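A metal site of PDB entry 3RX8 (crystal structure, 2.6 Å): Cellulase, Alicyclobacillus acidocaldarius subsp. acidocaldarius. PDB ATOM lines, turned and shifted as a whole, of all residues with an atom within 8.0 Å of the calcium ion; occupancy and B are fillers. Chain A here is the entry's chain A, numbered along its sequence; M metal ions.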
ATOM      1  N   VAL A 152       9.001  -4.348 -19.203  1.00  0.00           N
ATOM      2  CA  VAL A 152       8.854  -5.161 -20.402  1.00  0.00           C
ATOM      3  C   VAL A 152       9.447  -4.472 -21.664  1.00  0.00           C
ATOM      4  O   VAL A 152      10.416  -5.019 -22.183  1.00  0.00           O
ATOM      5  CB  VAL A 152       7.391  -5.699 -20.579  1.00  0.00           C
ATOM      6  CG1 VAL A 152       7.192  -6.337 -21.942  1.00  0.00           C
ATOM      7  CG2 VAL A 152       7.010  -6.653 -19.453  1.00  0.00           C
ATOM      8  N   ALA A 243       6.196 -11.618 -16.963  1.00  0.00           N
ATOM      9  CA  ALA A 243       6.806 -11.067 -18.150  1.00  0.00           C
ATOM     10  C   ALA A 243       7.932 -10.101 -17.823  1.00  0.00           C
ATOM     11  O   ALA A 243       9.020 -10.216 -18.415  1.00  0.00           O
ATOM     12  CB  ALA A 243       5.752 -10.372 -19.000  1.00  0.00           C
ATOM     13  N   THR A 247      11.525 -10.979 -19.037  1.00  0.00           N
ATOM     14  CA  THR A 247      12.237 -10.085 -19.977  1.00  0.00           C
ATOM     15  C   THR A 247      13.466  -9.477 -19.302  1.00  0.00           C
ATOM     16  O   THR A 247      14.484  -9.289 -19.969  1.00  0.00           O
ATOM     17  CB  THR A 247      11.325  -9.044 -20.566  1.00  0.00           C
ATOM     18  OG1 THR A 247      10.680  -8.358 -19.504  1.00  0.00           O
ATOM     19  CG2 THR A 247      10.305  -9.639 -21.525  1.00  0.00           C
ATOM     20  N   GLY A 301       0.431  -5.485 -21.637  1.00  0.00           N
ATOM     21  CA  GLY A 301      -0.079  -6.802 -21.324  1.00  0.00           C
ATOM     22  C   GLY A 301       0.231  -7.791 -22.432  1.00  0.00           C
ATOM     23  O   GLY A 301       0.438  -7.385 -23.589  1.00  0.00           O
ATOM     24  N   ASP A 302       0.230  -9.087 -22.088  1.00  0.00           N
ATOM     25  CA  ASP A 302       0.576 -10.181 -22.976  1.00  0.00           C
ATOM     26  C   ASP A 302       0.146 -11.485 -22.320  1.00  0.00           C
ATOM     27  O   ASP A 302       0.619 -11.841 -21.247  1.00  0.00           O
ATOM     28  CB  ASP A 302       2.097 -10.134 -23.233  1.00  0.00           C
ATOM     29  CG  ASP A 302       2.703 -11.168 -24.156  1.00  0.00           C
ATOM     30  OD1 ASP A 302       1.975 -11.681 -25.070  1.00  0.00           O
ATOM     31  OD2 ASP A 302       3.919 -11.436 -24.024  1.00  0.00           O
ATOM     32  N   ALA A 303      -0.792 -12.178 -22.967  1.00  0.00           N
ATOM     33  CA  ALA A 303      -1.372 -13.422 -22.493  1.00  0.00           C
ATOM     34  C   ALA A 303      -0.457 -14.596 -22.784  1.00  0.00           C
ATOM     35  O   ALA A 303      -0.604 -15.638 -22.143  1.00  0.00           O
ATOM     36  CB  ALA A 303      -2.703 -13.639 -23.167  1.00  0.00           C
ATOM     37  N   GLU A 304       0.485 -14.449 -23.736  1.00  0.00           N
ATOM     38  CA  GLU A 304       1.402 -15.509 -24.114  1.00  0.00           C
ATOM     39  C   GLU A 304       2.747 -15.244 -23.489  1.00  0.00           C
ATOM     40  O   GLU A 304       3.410 -14.271 -23.856  1.00  0.00           O
ATOM     41  CB  GLU A 304       1.509 -15.653 -25.644  1.00  0.00           C
ATOM     42  CG  GLU A 304       2.503 -16.718 -26.096  1.00  0.00           C
ATOM     43  CD  GLU A 304       2.361 -18.083 -25.432  1.00  0.00           C
ATOM     44  OE1 GLU A 304       1.398 -18.821 -25.749  1.00  0.00           O
ATOM     45  OE2 GLU A 304       3.225 -18.403 -24.596  1.00  0.00           O
ATOM     46  N   LEU A 305       3.155 -16.102 -22.509  1.00  0.00           N
ATOM     47  CA  LEU A 305       4.404 -15.888 -21.765  1.00  0.00           C
ATOM     48  C   LEU A 305       5.531 -16.914 -21.982  1.00  0.00           C
ATOM     49  O   LEU A 305       6.595 -16.777 -21.375  1.00  0.00           O
ATOM     50  CB  LEU A 305       4.111 -15.637 -20.264  1.00  0.00           C
ATOM     51  CG  LEU A 305       3.161 -14.456 -19.954  1.00  0.00           C
ATOM     52  CD1 LEU A 305       2.666 -14.496 -18.492  1.00  0.00           C
ATOM     53  CD2 LEU A 305       3.802 -13.114 -20.289  1.00  0.00           C
ATOM     54  N   ARG A 306       5.317 -17.896 -22.859  1.00  0.00           N
ATOM     55  CA  ARG A 306       6.319 -18.927 -23.146  1.00  0.00           C
ATOM     56  C   ARG A 306       7.468 -18.424 -23.988  1.00  0.00           C
ATOM     57  O   ARG A 306       8.593 -18.937 -23.868  1.00  0.00           O
ATOM     58  CB  ARG A 306       5.676 -20.139 -23.797  1.00  0.00           C
ATOM     59  CG  ARG A 306       4.839 -20.942 -22.831  1.00  0.00           C
ATOM     60  CD  ARG A 306       4.145 -22.037 -23.571  1.00  0.00           C
ATOM     61  NE  ARG A 306       3.172 -21.472 -24.496  1.00  0.00           N
ATOM     62  CZ  ARG A 306       2.446 -22.186 -25.348  1.00  0.00           C
ATOM     63  NH1 ARG A 306       2.624 -23.503 -25.445  1.00  0.00           N
ATOM     64  NH2 ARG A 306       1.549 -21.578 -26.130  1.00  0.00           N
ATOM     65  N   ASP A 307       7.188 -17.406 -24.851  1.00  0.00           N
ATOM     66  CA  ASP A 307       8.208 -16.754 -25.675  1.00  0.00           C
ATOM     67  C   ASP A 307       9.215 -15.973 -24.784  1.00  0.00           C
ATOM     68  O   ASP A 307      10.398 -15.909 -25.139  1.00  0.00           O
ATOM     69  CB  ASP A 307       7.562 -15.847 -26.731  1.00  0.00           C
ATOM     70  CG  ASP A 307       6.660 -14.775 -26.181  1.00  0.00           C
ATOM     71  OD1 ASP A 307       5.562 -15.104 -25.703  1.00  0.00           O
ATOM     72  OD2 ASP A 307       7.040 -13.596 -26.257  1.00  0.00           O
ATOM     73  N   GLU A 308       8.757 -15.417 -23.605  1.00  0.00           N
ATOM     74  CA  GLU A 308       9.597 -14.698 -22.626  1.00  0.00           C
ATOM     75  C   GLU A 308      10.489 -15.718 -21.883  1.00  0.00           C
ATOM     76  O   GLU A 308      11.673 -15.414 -21.633  1.00  0.00           O
ATOM     77  CB  GLU A 308       8.735 -13.950 -21.586  1.00  0.00           C
ATOM     78  CG  GLU A 308       8.102 -12.643 -22.056  1.00  0.00           C
ATOM     79  CD  GLU A 308       6.946 -12.770 -23.035  1.00  0.00           C
ATOM     80  OE1 GLU A 308       6.397 -13.890 -23.200  1.00  0.00           O
ATOM     81  OE2 GLU A 308       6.621 -11.742 -23.664  1.00  0.00           O
ATOM     82  N   LEU A 309       9.901 -16.910 -21.524  1.00  0.00           N
ATOM     83  CA  LEU A 309      10.640 -18.002 -20.862  1.00  0.00           C
ATOM     84  C   LEU A 309      11.765 -18.475 -21.808  1.00  0.00           C
ATOM     85  O   LEU A 309      12.914 -18.527 -21.374  1.00  0.00           O
ATOM     86  CB  LEU A 309       9.697 -19.153 -20.460  1.00  0.00           C
ATOM     87  CG  LEU A 309      10.299 -20.298 -19.625  1.00  0.00           C
ATOM     88  CD1 LEU A 309      10.808 -19.796 -18.214  1.00  0.00           C
ATOM     89  CD2 LEU A 309       9.297 -21.475 -19.479  1.00  0.00           C
ATOM     90  N   LEU A 337       5.235 -20.513 -31.619  1.00  0.00           N
ATOM     91  CA  LEU A 337       5.206 -19.115 -31.186  1.00  0.00           C
ATOM     92  C   LEU A 337       5.685 -18.223 -32.357  1.00  0.00           C
ATOM     93  O   LEU A 337       6.549 -18.652 -33.125  1.00  0.00           O
ATOM     94  CB  LEU A 337       6.161 -18.923 -29.999  1.00  0.00           C
ATOM     95  CG  LEU A 337       5.860 -19.697 -28.709  1.00  0.00           C
ATOM     96  CD1 LEU A 337       7.119 -19.898 -27.894  1.00  0.00           C
ATOM     97  CD2 LEU A 337       4.867 -18.966 -27.863  1.00  0.00           C
ATOM     98  N   PRO A 338       5.163 -16.982 -32.516  1.00  0.00           N
ATOM     99  CA  PRO A 338       5.690 -16.112 -33.593  1.00  0.00           C
ATOM    100  C   PRO A 338       7.157 -15.764 -33.322  1.00  0.00           C
ATOM    101  O   PRO A 338       7.481 -15.280 -32.227  1.00  0.00           O
ATOM    102  CB  PRO A 338       4.806 -14.852 -33.512  1.00  0.00           C
ATOM    103  CG  PRO A 338       3.702 -15.174 -32.570  1.00  0.00           C
ATOM    104  CD  PRO A 338       4.144 -16.287 -31.699  1.00  0.00           C
ATOM    105  N   GLY A 342       9.714  -8.521 -30.243  1.00  0.00           N
ATOM    106  CA  GLY A 342       9.071  -7.694 -29.234  1.00  0.00           C
ATOM    107  C   GLY A 342       8.070  -6.637 -29.685  1.00  0.00           C
ATOM    108  O   GLY A 342       7.774  -6.538 -30.874  1.00  0.00           O
ATOM    109  N   TRP A 343       7.535  -5.861 -28.731  1.00  0.00           N
ATOM    110  CA  TRP A 343       7.883  -5.966 -27.294  1.00  0.00           C
ATOM    111  C   TRP A 343       7.181  -7.149 -26.596  1.00  0.00           C
ATOM    112  O   TRP A 343       7.681  -7.613 -25.575  1.00  0.00           O
ATOM    113  CB  TRP A 343       7.572  -4.650 -26.559  1.00  0.00           C
ATOM    114  CG  TRP A 343       6.142  -4.237 -26.692  1.00  0.00           C
ATOM    115  CD1 TRP A 343       5.623  -3.410 -27.637  1.00  0.00           C
ATOM    116  CD2 TRP A 343       5.035  -4.729 -25.925  1.00  0.00           C
ATOM    117  NE1 TRP A 343       4.253  -3.332 -27.493  1.00  0.00           N
ATOM    118  CE2 TRP A 343       3.872  -4.131 -26.450  1.00  0.00           C
ATOM    119  CE3 TRP A 343       4.914  -5.588 -24.822  1.00  0.00           C
ATOM    120  CZ2 TRP A 343       2.598  -4.390 -25.927  1.00  0.00           C
ATOM    121  CZ3 TRP A 343       3.653  -5.832 -24.294  1.00  0.00           C
ATOM    122  CH2 TRP A 343       2.508  -5.256 -24.867  1.00  0.00           C
ATOM    123  N   ALA A 344       6.033  -7.640 -27.153  1.00  0.00           N
ATOM    124  CA  ALA A 344       5.242  -8.755 -26.578  1.00  0.00           C
ATOM    125  C   ALA A 344       5.642 -10.133 -27.070  1.00  0.00           C
ATOM    126  O   ALA A 344       5.578 -11.088 -26.307  1.00  0.00           O
ATOM    127  CB  ALA A 344       3.749  -8.516 -26.787  1.00  0.00           C
ATOM    128  N   ASP A 345       6.049 -10.249 -28.335  1.00  0.00           N
ATOM    129  CA  ASP A 345       6.463 -11.522 -28.912  1.00  0.00           C
ATOM    130  C   ASP A 345       7.983 -11.377 -29.111  1.00  0.00           C
ATOM    131  O   ASP A 345       8.446 -10.644 -29.988  1.00  0.00           O
ATOM    132  CB  ASP A 345       5.706 -11.786 -30.218  1.00  0.00           C
ATOM    133  CG  ASP A 345       4.205 -11.740 -30.031  1.00  0.00           C
ATOM    134  OD1 ASP A 345       3.591 -10.720 -30.431  1.00  0.00           O
ATOM    135  OD2 ASP A 345       3.656 -12.667 -29.404  1.00  0.00           O
ATOM    136  N   VAL A 346       8.750 -12.032 -28.219  1.00  0.00           N
ATOM    137  CA  VAL A 346      10.188 -11.922 -28.097  1.00  0.00           C
ATOM    138  C   VAL A 346      11.024 -13.146 -28.510  1.00  0.00           C
ATOM    139  O   VAL A 346      12.254 -13.077 -28.437  1.00  0.00           O
ATOM    140  CB  VAL A 346      10.554 -11.405 -26.669  1.00  0.00           C
ATOM    141  CG1 VAL A 346       9.973 -10.013 -26.420  1.00  0.00           C
ATOM    142  CG2 VAL A 346      10.100 -12.394 -25.578  1.00  0.00           C
ATOM    143  N   ALA A 347      10.371 -14.258 -28.887  1.00  0.00           N
ATOM    144  CA  ALA A 347      10.977 -15.521 -29.274  1.00  0.00           C
ATOM    145  C   ALA A 347      12.262 -15.408 -30.091  1.00  0.00           C
ATOM    146  O   ALA A 347      13.223 -16.097 -29.772  1.00  0.00           O
ATOM    147  CB  ALA A 347       9.959 -16.368 -30.013  1.00  0.00           C
HETATM  148 CA    CA M   1       5.032 -12.881 -25.010  1.00  0.00          CA
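The backbone NH (N) of Val 346 sits close to the side-chain carboxylate (OD2) of Asp 307 (3.0 Å). The guanidinium group (NH2) of Arg 306 lies within salt-bridge range of the side-chain carboxylate (OE1) of Glu 304, 2.8 Å away.
Within 4 Å of the calcium ion: Asp 302, Glu 304, Asp 307, Glu 308 and Ala 344. The nearest printed residue that does not touch the calcium ion is Asp 345 (4.4 Å).
The calcium ion is bound by OD2 of Asp 302, O of Ala 344, OE2 of Glu 308, OD1 of Asp 307, O of Glu 304, OD2 of Asp 307 and OE1 of Glu 308. The calcium ion has seven donor atoms within binding distance.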
